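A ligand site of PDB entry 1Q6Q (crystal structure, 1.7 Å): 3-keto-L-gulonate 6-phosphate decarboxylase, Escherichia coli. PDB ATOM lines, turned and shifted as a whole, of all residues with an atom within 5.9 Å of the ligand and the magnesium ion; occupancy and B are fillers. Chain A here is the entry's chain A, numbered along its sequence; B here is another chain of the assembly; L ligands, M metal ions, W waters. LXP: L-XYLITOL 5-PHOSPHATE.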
ATOM      1  N   ALA A   9      17.174  -8.972 -16.139  1.00  0.00           N
ATOM      2  CA  ALA A   9      18.266  -9.489 -16.963  1.00  0.00           C
ATOM      3  C   ALA A   9      18.873  -8.349 -17.738  1.00  0.00           C
ATOM      4  O   ALA A   9      18.233  -7.742 -18.585  1.00  0.00           O
ATOM      5  CB  ALA A   9      17.812 -10.611 -17.928  1.00  0.00           C
ATOM      6  N   ASP A  11      20.880  -8.127 -20.479  1.00  0.00           N
ATOM      7  CA  ASP A  11      21.407  -8.785 -21.673  1.00  0.00           C
ATOM      8  C   ASP A  11      21.773  -7.651 -22.607  1.00  0.00           C
ATOM      9  O   ASP A  11      21.141  -7.415 -23.626  1.00  0.00           O
ATOM     10  CB  ASP A  11      20.387  -9.725 -22.269  1.00  0.00           C
ATOM     11  CG  ASP A  11      20.234 -10.993 -21.445  1.00  0.00           C
ATOM     12  OD1 ASP A  11      21.292 -11.633 -21.141  1.00  0.00           O
ATOM     13  OD2 ASP A  11      19.120 -11.411 -21.125  1.00  0.00           O
ATOM     14  N   GLU A  33      20.806  -9.097 -12.753  1.00  0.00           N
ATOM     15  CA  GLU A  33      21.532 -10.095 -13.501  1.00  0.00           C
ATOM     16  C   GLU A  33      22.480  -9.421 -14.522  1.00  0.00           C
ATOM     17  O   GLU A  33      22.061  -8.653 -15.381  1.00  0.00           O
ATOM     18  CB  GLU A  33      20.585 -11.058 -14.194  1.00  0.00           C
ATOM     19  CG  GLU A  33      21.199 -11.773 -15.385  1.00  0.00           C
ATOM     20  CD  GLU A  33      20.244 -12.669 -16.157  1.00  0.00           C
ATOM     21  OE1 GLU A  33      19.141 -12.979 -15.597  1.00  0.00           O
ATOM     22  OE2 GLU A  33      20.606 -13.070 -17.293  1.00  0.00           O
ATOM     23  N   VAL A  34      23.709  -9.888 -14.499  1.00  0.00           N
ATOM     24  CA  VAL A  34      24.671  -9.660 -15.543  1.00  0.00           C
ATOM     25  C   VAL A  34      24.400 -10.777 -16.547  1.00  0.00           C
ATOM     26  O   VAL A  34      24.733 -11.922 -16.328  1.00  0.00           O
ATOM     27  CB  VAL A  34      26.117  -9.779 -14.975  1.00  0.00           C
ATOM     28  CG1 VAL A  34      27.147  -9.394 -16.080  1.00  0.00           C
ATOM     29  CG2 VAL A  34      26.236  -8.847 -13.754  1.00  0.00           C
ATOM     30  N   GLY A  35      23.712 -10.473 -17.629  1.00  0.00           N
ATOM     31  CA  GLY A  35      23.333 -11.462 -18.597  1.00  0.00           C
ATOM     32  C   GLY A  35      24.533 -12.052 -19.267  1.00  0.00           C
ATOM     33  O   GLY A  35      25.612 -11.461 -19.320  1.00  0.00           O
ATOM     34  N   THR A  36      24.285 -13.185 -19.905  1.00  0.00           N
ATOM     35  CA  THR A  36      25.353 -13.883 -20.617  1.00  0.00           C
ATOM     36  C   THR A  36      25.965 -12.968 -21.686  1.00  0.00           C
ATOM     37  O   THR A  36      27.182 -12.914 -21.817  1.00  0.00           O
ATOM     38  CB  THR A  36      24.836 -15.131 -21.234  1.00  0.00           C
ATOM     39  OG1 THR A  36      23.985 -15.814 -20.270  1.00  0.00           O
ATOM     40  CG2 THR A  36      26.031 -16.064 -21.553  1.00  0.00           C
ATOM     41  N   ILE A  37      25.108 -12.183 -22.357  1.00  0.00           N
ATOM     42  CA  ILE A  37      25.545 -11.270 -23.402  1.00  0.00           C
ATOM     43  C   ILE A  37      26.482 -10.212 -22.812  1.00  0.00           C
ATOM     44  O   ILE A  37      27.454  -9.824 -23.439  1.00  0.00           O
ATOM     45  CB  ILE A  37      24.273 -10.635 -24.072  1.00  0.00           C
ATOM     46  CG1 ILE A  37      23.667 -11.689 -25.012  1.00  0.00           C
ATOM     47  CG2 ILE A  37      24.586  -9.408 -24.856  1.00  0.00           C
ATOM     48  CD1 ILE A  37      22.143 -11.578 -25.275  1.00  0.00           C
ATOM     49  N   LEU A  60      23.583 -11.559  -9.869  1.00  0.00           N
ATOM     50  CA  LEU A  60      23.628 -12.872 -10.484  1.00  0.00           C
ATOM     51  C   LEU A  60      24.438 -12.759 -11.729  1.00  0.00           C
ATOM     52  O   LEU A  60      24.114 -11.947 -12.587  1.00  0.00           O
ATOM     53  CB  LEU A  60      22.170 -13.295 -10.796  1.00  0.00           C
ATOM     54  CG  LEU A  60      21.838 -14.634 -11.490  1.00  0.00           C
ATOM     55  CD1 LEU A  60      21.938 -14.543 -12.992  1.00  0.00           C
ATOM     56  CD2 LEU A  60      22.678 -15.821 -10.988  1.00  0.00           C
ATOM     57  N   ASP A  62      25.116 -14.478 -14.969  1.00  0.00           N
ATOM     58  CA  ASP A  62      24.527 -15.513 -15.827  1.00  0.00           C
ATOM     59  C   ASP A  62      25.589 -16.031 -16.828  1.00  0.00           C
ATOM     60  O   ASP A  62      25.449 -15.912 -18.042  1.00  0.00           O
ATOM     61  CB  ASP A  62      23.239 -15.003 -16.548  1.00  0.00           C
ATOM     62  CG  ASP A  62      22.411 -16.155 -17.163  1.00  0.00           C
ATOM     63  OD1 ASP A  62      22.761 -17.363 -16.977  1.00  0.00           O
ATOM     64  OD2 ASP A  62      21.481 -15.993 -17.937  1.00  0.00           O
ATOM     65  N   LYS A  64      26.547 -19.180 -17.339  1.00  0.00           N
ATOM     66  CA  LYS A  64      26.239 -20.449 -18.032  1.00  0.00           C
ATOM     67  C   LYS A  64      27.486 -21.348 -18.125  1.00  0.00           C
ATOM     68  O   LYS A  64      27.827 -21.920 -19.159  1.00  0.00           O
ATOM     69  CB  LYS A  64      25.556 -20.249 -19.386  1.00  0.00           C
ATOM     70  CG  LYS A  64      24.214 -19.479 -19.351  1.00  0.00           C
ATOM     71  CD  LYS A  64      23.529 -19.659 -20.681  1.00  0.00           C
ATOM     72  CE  LYS A  64      22.386 -18.709 -21.120  1.00  0.00           C
ATOM     73  NZ  LYS A  64      21.709 -18.151 -20.014  1.00  0.00           N
ATOM     74  N   GLU A 112      21.023 -23.881 -14.772  1.00  0.00           N
ATOM     75  CA  GLU A 112      20.170 -23.458 -15.875  1.00  0.00           C
ATOM     76  C   GLU A 112      19.610 -24.672 -16.612  1.00  0.00           C
ATOM     77  O   GLU A 112      20.371 -25.479 -17.173  1.00  0.00           O
ATOM     78  CB  GLU A 112      20.923 -22.581 -16.866  1.00  0.00           C
ATOM     79  CG  GLU A 112      19.911 -22.160 -17.931  1.00  0.00           C
ATOM     80  CD  GLU A 112      20.500 -21.522 -19.154  1.00  0.00           C
ATOM     81  OE1 GLU A 112      20.801 -20.312 -19.070  1.00  0.00           O
ATOM     82  OE2 GLU A 112      20.617 -22.221 -20.186  1.00  0.00           O
ATOM     83  N   HIS A 136      14.203 -22.349 -17.765  1.00  0.00           N
ATOM     84  CA  HIS A 136      14.768 -21.313 -18.737  1.00  0.00           C
ATOM     85  C   HIS A 136      14.277 -21.641 -20.135  1.00  0.00           C
ATOM     86  O   HIS A 136      14.899 -22.450 -20.850  1.00  0.00           O
ATOM     87  CB  HIS A 136      16.330 -21.341 -18.632  1.00  0.00           C
ATOM     88  CG  HIS A 136      17.070 -20.181 -19.279  1.00  0.00           C
ATOM     89  ND1 HIS A 136      17.023 -19.944 -20.632  1.00  0.00           N
ATOM     90  CD2 HIS A 136      18.012 -19.343 -18.800  1.00  0.00           C
ATOM     91  CE1 HIS A 136      17.725 -18.859 -20.925  1.00  0.00           C
ATOM     92  NE2 HIS A 136      18.364 -18.477 -19.817  1.00  0.00           N
ATOM     93  N   ARG A 137      13.179 -21.004 -20.563  1.00  0.00           N
ATOM     94  CA  ARG A 137      12.712 -21.154 -21.918  1.00  0.00           C
ATOM     95  C   ARG A 137      13.637 -20.407 -22.849  1.00  0.00           C
ATOM     96  O   ARG A 137      13.848 -19.225 -22.691  1.00  0.00           O
ATOM     97  CB  ARG A 137      11.233 -20.714 -22.042  1.00  0.00           C
ATOM     98  CG  ARG A 137      10.686 -20.714 -23.500  1.00  0.00           C
ATOM     99  CD  ARG A 137       9.195 -20.379 -23.586  1.00  0.00           C
ATOM    100  NE  ARG A 137       8.973 -18.965 -23.317  1.00  0.00           N
ATOM    101  CZ  ARG A 137       7.819 -18.427 -22.897  1.00  0.00           C
ATOM    102  NH1 ARG A 137       6.715 -19.186 -22.750  1.00  0.00           N
ATOM    103  NH2 ARG A 137       7.749 -17.135 -22.673  1.00  0.00           N
ATOM    104  N   ARG A 139      15.021 -18.308 -25.923  1.00  0.00           N
ATOM    105  CA  ARG A 139      14.440 -17.311 -26.797  1.00  0.00           C
ATOM    106  C   ARG A 139      14.473 -17.747 -28.224  1.00  0.00           C
ATOM    107  O   ARG A 139      13.720 -17.245 -29.026  1.00  0.00           O
ATOM    108  CB  ARG A 139      15.078 -15.917 -26.599  1.00  0.00           C
ATOM    109  CG  ARG A 139      16.344 -15.702 -27.346  1.00  0.00           C
ATOM    110  CD  ARG A 139      16.687 -14.268 -27.476  1.00  0.00           C
ATOM    111  NE  ARG A 139      16.897 -13.684 -26.174  1.00  0.00           N
ATOM    112  CZ  ARG A 139      17.246 -12.417 -25.975  1.00  0.00           C
ATOM    113  NH1 ARG A 139      17.384 -11.597 -26.999  1.00  0.00           N
ATOM    114  NH2 ARG A 139      17.458 -11.984 -24.732  1.00  0.00           N
ATOM    115  N   THR A 169      11.791 -18.021 -16.108  1.00  0.00           N
ATOM    116  CA  THR A 169      12.272 -17.056 -17.073  1.00  0.00           C
ATOM    117  C   THR A 169      12.220 -17.526 -18.527  1.00  0.00           C
ATOM    118  O   THR A 169      12.207 -18.736 -18.877  1.00  0.00           O
ATOM    119  CB  THR A 169      13.736 -16.692 -16.714  1.00  0.00           C
ATOM    120  OG1 THR A 169      14.116 -15.528 -17.487  1.00  0.00           O
ATOM    121  CG2 THR A 169      14.740 -17.827 -17.090  1.00  0.00           C
ATOM    122  N   GLY A 170      12.263 -16.546 -19.414  1.00  0.00           N
ATOM    123  CA  GLY A 170      12.447 -16.759 -20.826  1.00  0.00           C
ATOM    124  C   GLY A 170      11.296 -16.114 -21.558  1.00  0.00           C
ATOM    125  O   GLY A 170      10.269 -16.738 -21.775  1.00  0.00           O
ATOM    126  N   GLY A 171      11.519 -14.885 -22.003  1.00  0.00           N
ATOM    127  CA  GLY A 171      10.456 -14.068 -22.609  1.00  0.00           C
ATOM    128  C   GLY A 171       9.216 -13.845 -21.756  1.00  0.00           C
ATOM    129  O   GLY A 171       8.115 -13.678 -22.302  1.00  0.00           O
ATOM    130  N   LEU A 172       9.375 -13.793 -20.437  1.00  0.00           N
ATOM    131  CA  LEU A 172       8.251 -13.570 -19.540  1.00  0.00           C
ATOM    132  C   LEU A 172       7.609 -12.200 -19.744  1.00  0.00           C
ATOM    133  O   LEU A 172       8.296 -11.192 -19.926  1.00  0.00           O
ATOM    134  CB  LEU A 172       8.702 -13.631 -18.138  1.00  0.00           C
ATOM    135  CG  LEU A 172       7.642 -13.983 -17.160  1.00  0.00           C
ATOM    136  CD1 LEU A 172       7.152 -15.418 -17.479  1.00  0.00           C
ATOM    137  CD2 LEU A 172       8.261 -13.884 -15.776  1.00  0.00           C
ATOM    138  N   ILE A 189      12.272 -13.685 -13.630  1.00  0.00           N
ATOM    139  CA  ILE A 189      13.190 -12.799 -14.397  1.00  0.00           C
ATOM    140  C   ILE A 189      12.458 -12.148 -15.537  1.00  0.00           C
ATOM    141  O   ILE A 189      11.776 -12.831 -16.365  1.00  0.00           O
ATOM    142  CB  ILE A 189      14.351 -13.602 -15.019  1.00  0.00           C
ATOM    143  CG1 ILE A 189      15.093 -14.405 -13.966  1.00  0.00           C
ATOM    144  CG2 ILE A 189      15.318 -12.700 -15.746  1.00  0.00           C
ATOM    145  CD1 ILE A 189      16.215 -15.242 -14.593  1.00  0.00           C
ATOM    146  N   ALA A 190      12.646 -10.832 -15.676  1.00  0.00           N
ATOM    147  CA  ALA A 190      12.263 -10.109 -16.862  1.00  0.00           C
ATOM    148  C   ALA A 190      13.447  -9.374 -17.459  1.00  0.00           C
ATOM    149  O   ALA A 190      14.089  -8.601 -16.768  1.00  0.00           O
ATOM    150  CB  ALA A 190      11.161  -9.110 -16.533  1.00  0.00           C
ATOM    151  N   GLY A 191      13.710  -9.655 -18.712  1.00  0.00           N
ATOM    152  CA  GLY A 191      14.736  -8.948 -19.462  1.00  0.00           C
ATOM    153  C   GLY A 191      14.064  -7.945 -20.368  1.00  0.00           C
ATOM    154  O   GLY A 191      13.811  -6.827 -19.967  1.00  0.00           O
ATOM    155  N   ARG A 192      13.815  -8.375 -21.590  1.00  0.00           N
ATOM    156  CA  ARG A 192      13.181  -7.536 -22.616  1.00  0.00           C
ATOM    157  C   ARG A 192      11.909  -6.853 -22.099  1.00  0.00           C
ATOM    158  O   ARG A 192      11.690  -5.662 -22.339  1.00  0.00           O
ATOM    159  CB  ARG A 192      12.896  -8.354 -23.871  1.00  0.00           C
ATOM    160  CG  ARG A 192      14.171  -8.675 -24.636  1.00  0.00           C
ATOM    161  CD  ARG A 192      14.017  -9.745 -25.698  1.00  0.00           C
ATOM    162  NE  ARG A 192      13.786 -11.017 -25.049  1.00  0.00           N
ATOM    163  CZ  ARG A 192      13.271 -12.083 -25.646  1.00  0.00           C
ATOM    164  NH1 ARG A 192      13.104 -13.163 -24.958  1.00  0.00           N
ATOM    165  NH2 ARG A 192      12.982 -12.080 -26.944  1.00  0.00           N
ATOM    166  N   SER A 193      11.076  -7.582 -21.379  1.00  0.00           N
ATOM    167  CA  SER A 193       9.768  -7.027 -21.000  1.00  0.00           C
ATOM    168  C   SER A 193       9.877  -5.871 -20.000  1.00  0.00           C
ATOM    169  O   SER A 193       8.917  -5.108 -19.816  1.00  0.00           O
ATOM    170  CB  SER A 193       8.841  -8.154 -20.538  1.00  0.00           C
ATOM    171  OG  SER A 193       9.112  -8.491 -19.179  1.00  0.00           O
ATOM    172  N   ARG A 195      13.337  -3.966 -19.978  1.00  0.00           N
ATOM    173  CA  ARG A 195      14.295  -3.080 -20.634  1.00  0.00           C
ATOM    174  C   ARG A 195      13.656  -2.325 -21.798  1.00  0.00           C
ATOM    175  O   ARG A 195      13.993  -1.168 -22.068  1.00  0.00           O
ATOM    176  CB  ARG A 195      15.503  -3.842 -21.195  1.00  0.00           C
ATOM    177  CG  ARG A 195      16.353  -4.598 -20.134  1.00  0.00           C
ATOM    178  CD  ARG A 195      17.775  -4.816 -20.591  1.00  0.00           C
ATOM    179  NE  ARG A 195      17.764  -5.361 -21.964  1.00  0.00           N
ATOM    180  CZ  ARG A 195      17.597  -6.669 -22.255  1.00  0.00           C
ATOM    181  NH1 ARG A 195      17.507  -7.541 -21.252  1.00  0.00           N
ATOM    182  NH2 ARG A 195      17.485  -7.085 -23.510  1.00  0.00           N
ATOM    183  N   ASP B  67      22.262 -20.047 -25.988  1.00  0.00           N
ATOM    184  CA  ASP B  67      20.979 -19.337 -26.238  1.00  0.00           C
ATOM    185  C   ASP B  67      21.318 -18.018 -26.879  1.00  0.00           C
ATOM    186  O   ASP B  67      22.487 -17.616 -26.862  1.00  0.00           O
ATOM    187  CB  ASP B  67      20.258 -19.147 -24.912  1.00  0.00           C
ATOM    188  CG  ASP B  67      18.819 -18.658 -25.088  1.00  0.00           C
ATOM    189  OD1 ASP B  67      18.195 -18.856 -26.170  1.00  0.00           O
ATOM    190  OD2 ASP B  67      18.280 -18.054 -24.173  1.00  0.00           O
ATOM    191  N   ALA B  68      20.312 -17.343 -27.451  1.00  0.00           N
ATOM    192  CA  ALA B  68      20.514 -16.081 -28.149  1.00  0.00           C
ATOM    193  C   ALA B  68      21.625 -16.175 -29.157  1.00  0.00           C
ATOM    194  O   ALA B  68      22.536 -15.327 -29.212  1.00  0.00           O
ATOM    195  CB  ALA B  68      20.759 -14.950 -27.149  1.00  0.00           C
HETATM  196  O8  LXP L   1      13.989 -13.441 -22.107  1.00  0.00           O
HETATM  197  P   LXP L   1      14.169 -12.145 -21.369  1.00  0.00           P
HETATM  198  O6  LXP L   1      14.542 -11.064 -22.339  1.00  0.00           O
HETATM  199  O7  LXP L   1      13.105 -11.859 -20.337  1.00  0.00           O
HETATM  200  O5  LXP L   1      15.562 -12.319 -20.505  1.00  0.00           O
HETATM  201  C5  LXP L   1      15.692 -13.255 -19.455  1.00  0.00           C
HETATM  202  C4  LXP L   1      16.357 -14.494 -19.961  1.00  0.00           C
HETATM  203  O4  LXP L   1      16.457 -15.329 -18.808  1.00  0.00           O
HETATM  204  C3  LXP L   1      17.727 -14.201 -20.554  1.00  0.00           C
HETATM  205  O3  LXP L   1      18.566 -13.548 -19.607  1.00  0.00           O
HETATM  206  C2  LXP L   1      18.422 -15.536 -20.981  1.00  0.00           C
HETATM  207  O2  LXP L   1      19.212 -16.092 -19.883  1.00  0.00           O
HETATM  208  C1  LXP L   1      19.201 -15.350 -22.277  1.00  0.00           C
HETATM  209  O1  LXP L   1      20.060 -16.490 -22.563  1.00  0.00           O
HETATM  210 MG    MG M   1      20.131 -14.612 -18.554  1.00  0.00          MG
HETATM  211  O   HOH W   1      18.662 -15.129 -17.113  1.00  0.00           O
HETATM  212  O   HOH W   2      21.500 -13.918 -20.040  1.00  0.00           O
HETATM  213  O   HOH W   3      17.091 -10.195 -22.347  1.00  0.00           O
HETATM  214  O   HOH W   4      11.828 -13.735 -19.055  1.00  0.00           O
HETATM  215  O   HOH W   5      16.012 -14.534 -23.472  1.00  0.00           O
HETATM  216  O   HOH W   6      22.902 -16.450 -24.015  1.00  0.00           O
HETATM  217  O   HOH W   7      10.841 -10.590 -21.168  1.00  0.00           O
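The magnesium ion is bound by the side-chain carboxylate (OD2) of Asp 62, at 2.0 Å.
The side-chain carboxylate (OE2) of Glu 33 is bound to the magnesium ion, at 2.0 Å.
Water W1 is bound to the magnesium ion (2.1 Å).
Water W2 binds the magnesium ion (2.1 Å).
An oxygen (O3) of the ligand binds the magnesium ion (2.2 Å).
O2 of the ligand is bound to the magnesium ion.
The nearest printed residue that does not touch the magnesium ion is Asp 11 (4.1 Å).
Water W2 lies within hydrogen-bond range of OD1 of Asp 11 (2.5 Å) and N of Thr 36 (2.9 Å).
Water W1 bridges OE1 of Glu 33 (2.7 Å) and O4 of the ligand (2.8 Å).
Water W5 lies within hydrogen-bond range of O8 of the ligand (2.7 Å) and NE of Arg 139 (3.0 Å).
Water W3 lies within hydrogen-bond range of the side-chain carboxylate of Asp 11 (2.7 Å), an oxygen (O6) of the ligand (2.7 Å), the guanidinium group of Arg 195 (2.9 Å) and the guanidinium group of Arg 139 (3.0 Å).
Water W7 lies within hydrogen-bond range of an oxygen (O7) of the ligand (2.7 Å), the backbone carbonyl oxygen (O) of Leu 172 (2.9 Å) and the backbone NH (N) of Ser 193 (3.0 Å).
Water W6 lies within hydrogen-bond range of O of Asp 67 of chain B and O1 of the ligand.
Merely in contact with the ligand: Ala 9 (3.5 Å), Ile 189 (3.8 Å), Ala 190 (3.8 Å) and Gly 170 (3.8 Å).
Along chain A the residues within 4 Å of the ligand span positions 9 to 192.
The nearest printed residue that does not touch the ligand is Leu 172 (4.2 Å).
OD2 of Asp 67 of chain B sits at hydrogen-bond distance from O1 of the ligand, 2.9 Å away.
O8 of the ligand lies within hydrogen-bond range of N of Gly 171, 2.9 Å away.
NZ of Lys 64 sits at hydrogen-bond distance from O1 of the ligand (3.5 Å).
O7 of the ligand lies within hydrogen-bond range of N of Gly 191 (2.8 Å).
N of Arg 192 lies within hydrogen-bond range of O6 of the ligand, at 2.9 Å.
An oxygen (O2) of the ligand lies close to a ring nitrogen (NE2) of His 136.
The side-chain carboxylate (OD2) of Asp 11 sits close to an oxygen (O3) of the ligand, at 2.7 Å.
An oxygen (O6) of the ligand lies within salt-bridge range of the guanidinium group of Arg 139 (3.9 Å).
O4 of the ligand is in hydrogen-bond range of OG1 of Thr 169 (2.7 Å).
An oxygen (O6) of the ligand lies within salt-bridge range of the guanidinium group of Arg 192, 2.8 Å away.
A ring nitrogen (NE2) of His 136 lies within hydrogen-bond range of the side-chain amino group (NZ) of Lys 64 (3.4 Å).
The backbone carbonyl oxygen (O) of Asp 62 is in hydrogen-bond range of the side-chain hydroxyl (OG1) of Thr 36 (2.7 Å).
The backbone carbonyl oxygen of Gly 170 is in hydrogen-bond range of the guanidinium group of Arg 137 (2.7 Å).
The backbone carbonyl oxygen (O) of Ala 9 lies within hydrogen-bond range of the guanidinium group (NH1) of Arg 195.
OE1 of Glu 112 is in salt-bridge range of NZ of Lys 64, at 2.5 Å.
N of Asp 62 is in hydrogen-bond range of O of Val 34.
A ring nitrogen (NE2) of His 136 sits close to the side-chain carboxylate of Glu 112, 3.1 Å away.
N of Ala 9 is in hydrogen-bond range of O of Ala 190.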
